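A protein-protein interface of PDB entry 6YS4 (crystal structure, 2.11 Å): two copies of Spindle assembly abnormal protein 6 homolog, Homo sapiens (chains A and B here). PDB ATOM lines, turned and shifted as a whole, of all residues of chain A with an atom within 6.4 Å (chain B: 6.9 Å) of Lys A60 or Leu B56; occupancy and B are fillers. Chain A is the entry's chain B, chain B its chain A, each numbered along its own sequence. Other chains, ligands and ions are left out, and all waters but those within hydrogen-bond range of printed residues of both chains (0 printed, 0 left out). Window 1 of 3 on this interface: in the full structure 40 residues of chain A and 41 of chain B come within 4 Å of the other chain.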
ATOM      1  N   ALA A  52      -0.388 -25.108 -17.524  1.00  0.00           N
ATOM      2  CA  ALA A  52       0.032 -23.883 -16.861  1.00  0.00           C
ATOM      3  C   ALA A  52       1.314 -24.147 -16.048  1.00  0.00           C
ATOM      4  O   ALA A  52       2.186 -23.299 -16.013  1.00  0.00           O
ATOM      5  CB  ALA A  52      -1.077 -23.337 -15.963  1.00  0.00           C
ATOM      6  N   ASN A  53       1.449 -25.324 -15.436  1.00  0.00           N
ATOM      7  CA  ASN A  53       2.623 -25.675 -14.659  1.00  0.00           C
ATOM      8  C   ASN A  53       3.832 -25.865 -15.554  1.00  0.00           C
ATOM      9  O   ASN A  53       4.918 -25.449 -15.171  1.00  0.00           O
ATOM     10  CB  ASN A  53       2.382 -26.926 -13.802  1.00  0.00           C
ATOM     11  CG  ASN A  53       3.550 -27.317 -12.954  1.00  0.00           C
ATOM     12  OD1 ASN A  53       4.385 -28.126 -13.355  1.00  0.00           O
ATOM     13  ND2 ASN A  53       3.637 -26.740 -11.764  1.00  0.00           N
ATOM     14  N   ASP A  55       4.304 -24.347 -18.445  1.00  0.00           N
ATOM     15  CA  ASP A  55       4.626 -22.992 -18.875  1.00  0.00           C
ATOM     16  C   ASP A  55       5.372 -22.223 -17.770  1.00  0.00           C
ATOM     17  O   ASP A  55       6.370 -21.545 -18.066  1.00  0.00           O
ATOM     18  CB  ASP A  55       3.356 -22.253 -19.325  1.00  0.00           C
ATOM     19  CG  ASP A  55       3.609 -20.828 -19.788  1.00  0.00           C
ATOM     20  OD1 ASP A  55       4.328 -20.649 -20.812  1.00  0.00           O
ATOM     21  OD2 ASP A  55       3.093 -19.882 -19.128  1.00  0.00           O
ATOM     22  N   LEU A  56       4.947 -22.392 -16.503  1.00  0.00           N
ATOM     23  CA  LEU A  56       5.585 -21.733 -15.378  1.00  0.00           C
ATOM     24  C   LEU A  56       6.965 -22.219 -15.114  1.00  0.00           C
ATOM     25  O   LEU A  56       7.805 -21.411 -14.748  1.00  0.00           O
ATOM     26  CB  LEU A  56       4.753 -21.790 -14.103  1.00  0.00           C
ATOM     27  CG  LEU A  56       3.565 -20.795 -14.025  1.00  0.00           C
ATOM     28  CD1 LEU A  56       2.545 -21.279 -12.998  1.00  0.00           C
ATOM     29  CD2 LEU A  56       4.033 -19.341 -13.744  1.00  0.00           C
ATOM     30  N   THR A  57       7.202 -23.532 -15.254  1.00  0.00           N
ATOM     31  CA  THR A  57       8.486 -24.163 -15.003  1.00  0.00           C
ATOM     32  C   THR A  57       9.494 -23.707 -16.062  1.00  0.00           C
ATOM     33  O   THR A  57      10.647 -23.468 -15.733  1.00  0.00           O
ATOM     34  CB  THR A  57       8.359 -25.675 -14.833  1.00  0.00           C
ATOM     35  OG1 THR A  57       7.832 -26.220 -16.034  1.00  0.00           O
ATOM     36  CG2 THR A  57       7.509 -26.049 -13.608  1.00  0.00           C
ATOM     37  N   GLU A  58       9.025 -23.517 -17.310  1.00  0.00           N
ATOM     38  CA  GLU A  58       9.836 -23.005 -18.417  1.00  0.00           C
ATOM     39  C   GLU A  58      10.220 -21.555 -18.208  1.00  0.00           C
ATOM     40  O   GLU A  58      11.332 -21.190 -18.511  1.00  0.00           O
ATOM     41  CB  GLU A  58       9.114 -23.201 -19.754  1.00  0.00           C
ATOM     42  CG  GLU A  58       9.492 -24.522 -20.416  1.00  0.00           C
ATOM     43  CD  GLU A  58       8.412 -25.268 -21.179  1.00  0.00           C
ATOM     44  OE1 GLU A  58       7.424 -24.619 -21.595  1.00  0.00           O
ATOM     45  OE2 GLU A  58       8.567 -26.499 -21.380  1.00  0.00           O
ATOM     46  N   ARG A  59       9.308 -20.733 -17.655  1.00  0.00           N
ATOM     47  CA  ARG A  59       9.561 -19.325 -17.366  1.00  0.00           C
ATOM     48  C   ARG A  59      10.503 -19.184 -16.179  1.00  0.00           C
ATOM     49  O   ARG A  59      11.348 -18.294 -16.185  1.00  0.00           O
ATOM     50  CB  ARG A  59       8.261 -18.527 -17.165  1.00  0.00           C
ATOM     51  CG  ARG A  59       7.585 -18.146 -18.466  1.00  0.00           C
ATOM     52  CD  ARG A  59       6.086 -18.010 -18.225  1.00  0.00           C
ATOM     53  NE  ARG A  59       5.424 -17.076 -19.130  1.00  0.00           N
ATOM     54  CZ  ARG A  59       4.217 -16.571 -18.901  1.00  0.00           C
ATOM     55  NH1 ARG A  59       3.545 -16.900 -17.804  1.00  0.00           N
ATOM     56  NH2 ARG A  59       3.675 -15.724 -19.770  1.00  0.00           N
ATOM     57  N   LYS A  60      10.385 -20.086 -15.194  1.00  0.00           N
ATOM     58  CA  LYS A  60      11.252 -20.121 -14.023  1.00  0.00           C
ATOM     59  C   LYS A  60      12.698 -20.451 -14.473  1.00  0.00           C
ATOM     60  O   LYS A  60      13.632 -19.818 -13.984  1.00  0.00           O
ATOM     61  CB  LYS A  60      10.762 -21.146 -13.003  1.00  0.00           C
ATOM     62  CG  LYS A  60      11.515 -21.043 -11.687  1.00  0.00           C
ATOM     63  CD  LYS A  60      11.420 -22.282 -10.862  1.00  0.00           C
ATOM     64  CE  LYS A  60      12.210 -22.146  -9.585  1.00  0.00           C
ATOM     65  NZ  LYS A  60      13.657 -22.430  -9.795  1.00  0.00           N
ATOM     66  N   TYR A  61      12.876 -21.370 -15.446  1.00  0.00           N
ATOM     67  CA  TYR A  61      14.197 -21.695 -15.966  1.00  0.00           C
ATOM     68  C   TYR A  61      14.837 -20.479 -16.694  1.00  0.00           C
ATOM     69  O   TYR A  61      16.021 -20.179 -16.487  1.00  0.00           O
ATOM     70  CB  TYR A  61      14.172 -22.939 -16.882  1.00  0.00           C
ATOM     71  CG  TYR A  61      15.509 -23.142 -17.566  1.00  0.00           C
ATOM     72  CD1 TYR A  61      16.591 -23.695 -16.879  1.00  0.00           C
ATOM     73  CD2 TYR A  61      15.724 -22.691 -18.867  1.00  0.00           C
ATOM     74  CE1 TYR A  61      17.870 -23.755 -17.460  1.00  0.00           C
ATOM     75  CE2 TYR A  61      16.996 -22.735 -19.454  1.00  0.00           C
ATOM     76  CZ  TYR A  61      18.053 -23.290 -18.753  1.00  0.00           C
ATOM     77  OH  TYR A  61      19.250 -23.381 -19.364  1.00  0.00           O
ATOM     78  N   LYS A  62      14.029 -19.805 -17.539  1.00  0.00           N
ATOM     79  CA  LYS A  62      14.440 -18.650 -18.320  1.00  0.00           C
ATOM     80  C   LYS A  62      14.807 -17.476 -17.459  1.00  0.00           C
ATOM     81  O   LYS A  62      15.830 -16.874 -17.720  1.00  0.00           O
ATOM     82  CB  LYS A  62      13.400 -18.270 -19.387  1.00  0.00           C
ATOM     83  CG  LYS A  62      13.302 -19.276 -20.535  1.00  0.00           C
ATOM     84  CD  LYS A  62      14.505 -19.255 -21.497  1.00  0.00           C
ATOM     85  CE  LYS A  62      14.360 -20.239 -22.641  1.00  0.00           C
ATOM     86  NZ  LYS A  62      14.720 -21.626 -22.239  1.00  0.00           N
ATOM     87  N   GLY A  63      13.983 -17.162 -16.459  1.00  0.00           N
ATOM     88  CA  GLY A  63      14.246 -16.108 -15.494  1.00  0.00           C
ATOM     89  C   GLY A  63      15.516 -16.373 -14.707  1.00  0.00           C
ATOM     90  O   GLY A  63      16.366 -15.495 -14.634  1.00  0.00           O
ATOM     91  N   ASP A  64      15.664 -17.582 -14.120  1.00  0.00           N
ATOM     92  CA  ASP A  64      16.794 -17.967 -13.275  1.00  0.00           C
ATOM     93  C   ASP A  64      18.100 -17.985 -14.020  1.00  0.00           C
ATOM     94  O   ASP A  64      19.128 -17.663 -13.429  1.00  0.00           O
ATOM     95  CB  ASP A  64      16.595 -19.345 -12.653  1.00  0.00           C
ATOM     96  CG  ASP A  64      15.491 -19.497 -11.608  1.00  0.00           C
ATOM     97  OD1 ASP A  64      14.886 -18.460 -11.204  1.00  0.00           O
ATOM     98  OD2 ASP A  64      15.224 -20.647 -11.200  1.00  0.00           O
ATOM     99  N   SER A  65      18.073 -18.474 -15.279  1.00  0.00           N
ATOM    100  CA  SER A  65      19.244 -18.537 -16.145  1.00  0.00           C
ATOM    101  C   SER A  65      19.656 -17.130 -16.540  1.00  0.00           C
ATOM    102  O   SER A  65      20.842 -16.862 -16.512  1.00  0.00           O
ATOM    103  CB  SER A  65      18.973 -19.408 -17.362  1.00  0.00           C
ATOM    104  OG  SER A  65      20.147 -19.602 -18.123  1.00  0.00           O
ATOM    105  N   LEU B  49      -1.828 -28.777  -7.387  1.00  0.00           N
ATOM    106  CA  LEU B  49      -1.266 -28.193  -8.594  1.00  0.00           C
ATOM    107  C   LEU B  49      -1.621 -26.709  -8.727  1.00  0.00           C
ATOM    108  O   LEU B  49      -0.789 -25.952  -9.219  1.00  0.00           O
ATOM    109  CB  LEU B  49      -1.681 -28.969  -9.846  1.00  0.00           C
ATOM    110  CG  LEU B  49      -0.784 -28.815 -11.118  1.00  0.00           C
ATOM    111  CD1 LEU B  49       0.729 -28.688 -10.811  1.00  0.00           C
ATOM    112  CD2 LEU B  49      -0.950 -29.979 -12.012  1.00  0.00           C
ATOM    113  N   ALA B  51      -2.021 -24.677  -6.071  1.00  0.00           N
ATOM    114  CA  ALA B  51      -1.181 -24.024  -5.070  1.00  0.00           C
ATOM    115  C   ALA B  51       0.273 -23.937  -5.531  1.00  0.00           C
ATOM    116  O   ALA B  51       0.901 -22.895  -5.342  1.00  0.00           O
ATOM    117  CB  ALA B  51      -1.286 -24.738  -3.757  1.00  0.00           C
ATOM    118  N   ALA B  52       0.787 -24.987  -6.193  1.00  0.00           N
ATOM    119  CA  ALA B  52       2.154 -24.987  -6.752  1.00  0.00           C
ATOM    120  C   ALA B  52       2.266 -23.918  -7.846  1.00  0.00           C
ATOM    121  O   ALA B  52       3.282 -23.244  -7.923  1.00  0.00           O
ATOM    122  CB  ALA B  52       2.505 -26.369  -7.323  1.00  0.00           C
ATOM    123  N   ASN B  53       1.197 -23.748  -8.658  1.00  0.00           N
ATOM    124  CA  ASN B  53       1.158 -22.740  -9.726  1.00  0.00           C
ATOM    125  C   ASN B  53       1.130 -21.333  -9.164  1.00  0.00           C
ATOM    126  O   ASN B  53       1.804 -20.481  -9.709  1.00  0.00           O
ATOM    127  CB  ASN B  53       0.030 -22.978 -10.699  1.00  0.00           C
ATOM    128  CG  ASN B  53       0.267 -24.177 -11.611  1.00  0.00           C
ATOM    129  OD1 ASN B  53       1.328 -24.828 -11.597  1.00  0.00           O
ATOM    130  ND2 ASN B  53      -0.734 -24.521 -12.410  1.00  0.00           N
ATOM    131  N   LYS B  54       0.405 -21.112  -8.047  1.00  0.00           N
ATOM    132  CA  LYS B  54       0.326 -19.817  -7.377  1.00  0.00           C
ATOM    133  C   LYS B  54       1.714 -19.443  -6.861  1.00  0.00           C
ATOM    134  O   LYS B  54       2.141 -18.299  -7.020  1.00  0.00           O
ATOM    135  CB  LYS B  54      -0.705 -19.847  -6.236  1.00  0.00           C
ATOM    136  CG  LYS B  54      -0.887 -18.496  -5.554  1.00  0.00           C
ATOM    137  CD  LYS B  54      -1.701 -18.564  -4.259  1.00  0.00           C
ATOM    138  CE  LYS B  54      -1.615 -17.271  -3.463  1.00  0.00           C
ATOM    139  NZ  LYS B  54      -0.238 -16.981  -2.944  1.00  0.00           N
ATOM    140  N   ASP B  55       2.422 -20.420  -6.271  1.00  0.00           N
ATOM    141  CA  ASP B  55       3.782 -20.232  -5.767  1.00  0.00           C
ATOM    142  C   ASP B  55       4.774 -19.936  -6.878  1.00  0.00           C
ATOM    143  O   ASP B  55       5.589 -19.018  -6.732  1.00  0.00           O
ATOM    144  CB  ASP B  55       4.207 -21.415  -4.892  1.00  0.00           C
ATOM    145  CG  ASP B  55       3.513 -21.413  -3.513  1.00  0.00           C
ATOM    146  OD1 ASP B  55       3.619 -20.384  -2.778  1.00  0.00           O
ATOM    147  OD2 ASP B  55       2.855 -22.419  -3.176  1.00  0.00           O
ATOM    148  N   LEU B  56       4.654 -20.624  -8.021  1.00  0.00           N
ATOM    149  CA  LEU B  56       5.536 -20.362  -9.173  1.00  0.00           C
ATOM    150  C   LEU B  56       5.322 -18.972  -9.787  1.00  0.00           C
ATOM    151  O   LEU B  56       6.296 -18.339 -10.214  1.00  0.00           O
ATOM    152  CB  LEU B  56       5.360 -21.421 -10.275  1.00  0.00           C
ATOM    153  CG  LEU B  56       6.072 -22.748 -10.081  1.00  0.00           C
ATOM    154  CD1 LEU B  56       5.441 -23.815 -10.935  1.00  0.00           C
ATOM    155  CD2 LEU B  56       7.587 -22.620 -10.396  1.00  0.00           C
ATOM    156  N   THR B  57       4.046 -18.522  -9.880  1.00  0.00           N
ATOM    157  CA  THR B  57       3.705 -17.221 -10.441  1.00  0.00           C
ATOM    158  C   THR B  57       4.298 -16.103  -9.546  1.00  0.00           C
ATOM    159  O   THR B  57       4.840 -15.113 -10.058  1.00  0.00           O
ATOM    160  CB  THR B  57       2.183 -17.063 -10.675  1.00  0.00           C
ATOM    161  OG1 THR B  57       1.491 -17.257  -9.462  1.00  0.00           O
ATOM    162  CG2 THR B  57       1.623 -17.999 -11.713  1.00  0.00           C
ATOM    163  N   GLU B  58       4.222 -16.303  -8.211  1.00  0.00           N
ATOM    164  CA  GLU B  58       4.768 -15.408  -7.198  1.00  0.00           C
ATOM    165  C   GLU B  58       6.299 -15.319  -7.358  1.00  0.00           C
ATOM    166  O   GLU B  58       6.850 -14.218  -7.402  1.00  0.00           O
ATOM    167  CB  GLU B  58       4.347 -15.901  -5.799  1.00  0.00           C
ATOM    168  CG  GLU B  58       5.219 -15.421  -4.641  1.00  0.00           C
ATOM    169  CD  GLU B  58       6.328 -16.361  -4.192  1.00  0.00           C
ATOM    170  OE1 GLU B  58       6.022 -17.527  -3.846  1.00  0.00           O
ATOM    171  OE2 GLU B  58       7.503 -15.923  -4.171  1.00  0.00           O
ATOM    172  N   ARG B  59       6.965 -16.481  -7.501  1.00  0.00           N
ATOM    173  CA  ARG B  59       8.414 -16.615  -7.691  1.00  0.00           C
ATOM    174  C   ARG B  59       8.876 -15.903  -8.974  1.00  0.00           C
ATOM    175  O   ARG B  59       9.946 -15.272  -8.979  1.00  0.00           O
ATOM    176  CB  ARG B  59       8.827 -18.111  -7.721  1.00  0.00           C
ATOM    177  CG  ARG B  59       8.756 -18.867  -6.381  1.00  0.00           C
ATOM    178  CD  ARG B  59       9.944 -18.587  -5.488  1.00  0.00           C
ATOM    179  NE  ARG B  59      10.056 -19.530  -4.373  1.00  0.00           N
ATOM    180  CZ  ARG B  59      10.826 -20.617  -4.371  1.00  0.00           C
ATOM    181  NH1 ARG B  59      11.545 -20.928  -5.447  1.00  0.00           N
ATOM    182  NH2 ARG B  59      10.881 -21.402  -3.303  1.00  0.00           N
ATOM    183  N   LYS B  60       8.064 -16.005 -10.052  1.00  0.00           N
ATOM    184  CA  LYS B  60       8.335 -15.410 -11.364  1.00  0.00           C
ATOM    185  C   LYS B  60       8.371 -13.878 -11.247  1.00  0.00           C
ATOM    186  O   LYS B  60       9.289 -13.266 -11.791  1.00  0.00           O
ATOM    187  CB  LYS B  60       7.305 -15.878 -12.418  1.00  0.00           C
ATOM    188  CG  LYS B  60       7.560 -15.352 -13.837  1.00  0.00           C
ATOM    189  CD  LYS B  60       6.264 -14.877 -14.523  1.00  0.00           C
ATOM    190  CE  LYS B  60       6.481 -14.490 -15.971  1.00  0.00           C
ATOM    191  NZ  LYS B  60       7.242 -13.222 -16.154  1.00  0.00           N
ATOM    192  N   TYR B  61       7.374 -13.277 -10.540  1.00  0.00           N
ATOM    193  CA  TYR B  61       7.314 -11.840 -10.316  1.00  0.00           C
ATOM    194  C   TYR B  61       8.546 -11.330  -9.562  1.00  0.00           C
ATOM    195  O   TYR B  61       9.094 -10.311  -9.956  1.00  0.00           O
ATOM    196  CB  TYR B  61       5.990 -11.406  -9.655  1.00  0.00           C
ATOM    197  CG  TYR B  61       4.761 -11.653 -10.514  1.00  0.00           C
ATOM    198  CD1 TYR B  61       4.696 -11.191 -11.832  1.00  0.00           C
ATOM    199  CD2 TYR B  61       3.639 -12.301  -9.993  1.00  0.00           C
ATOM    200  CE1 TYR B  61       3.574 -11.434 -12.628  1.00  0.00           C
ATOM    201  CE2 TYR B  61       2.508 -12.541 -10.778  1.00  0.00           C
ATOM    202  CZ  TYR B  61       2.480 -12.104 -12.093  1.00  0.00           C
ATOM    203  OH  TYR B  61       1.365 -12.344 -12.857  1.00  0.00           O
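ND2 of Asn A53 sits at hydrogen-bond distance from OD1 of Asn B53, 3.0 Å away.
OD1 of Asn B53 lies close to O of Leu B49 (3.4 Å).
The side-chain hydroxyl of Thr B57 sits close to the backbone carbonyl oxygen of Asn B53, at 3.2 Å.
O of Lys B54 is in hydrogen-bond range of OG1 of Thr B57, at 2.7 Å.
OG1 of Thr A57 sits close to O of Asn A53 (3.1 Å).
OD2 of Asp A64 lies within salt-bridge range of NZ of Lys A60 (2.8 Å).
Among the printed residues, pairs that only touch across the chains: Ala A52 with Asn B53 (3.8 Å), Asn A53 with Leu B49 (3.6 Å), Asn A53 with Leu B56 (3.5 Å), Leu A56 with Asn B53 (3.5 Å), Leu A56 with Leu B56 (3.8 Å), Leu A56 with Thr B57 (3.4 Å) and Lys A60 with Leu B56 (3.9 Å).
Printed residues of chain B within 4 Å of Ala A52: Asn B53.
Printed residues of chain B within 4 Å of Leu A56: Asn B53, Leu B56 and Thr B57.
Lys A60 touches one residue of chain B.
Of the printed residues of chain A, Leu B49 touches Asn A53 (3.6 Å).
Of the printed residues of chain A, Leu B56 touches Asn A53 (3.5 Å), Leu A56 (3.8 Å) and Lys A60 (3.9 Å).
Of the printed residues of chain A, Thr B57 touches Leu A56.
The nearest residue of chain A that does not touch Leu B56 is Thr A57 (4.1 Å).
Of the 13 printed residues of chain A, 4 touch a printed residue of chain B.
Hydrophobic or aromatic side chains of chain A within 4 Å of the printed part of chain B: Ala A52 and Leu A56.
Of the 12 printed residues of chain B, 4 touch a printed residue of chain A.
Hydrophobic or aromatic side chains of chain B that line the printed part of chain A: Leu B49 and Leu B56.
Along chain B the printed residues that touch a printed residue of chain A span positions 49 to 57.
Among the printed residues, 8 pairs touch across the chains.
Ala A52 touches Asn B53, but with the chains exchanged Asn A53 does not touch Ala B52 (4.6 Å).
Asn B53 touches its own counterpart, Asn A53.
Leu A56 touches Thr B57, but with the chains exchanged Thr A57 does not touch Leu B56 (4.1 Å).
Lys A60 touches Leu B56, but with the chains exchanged Leu A56 does not touch Lys B60 (4.9 Å).
9 positions are printed for both chains.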
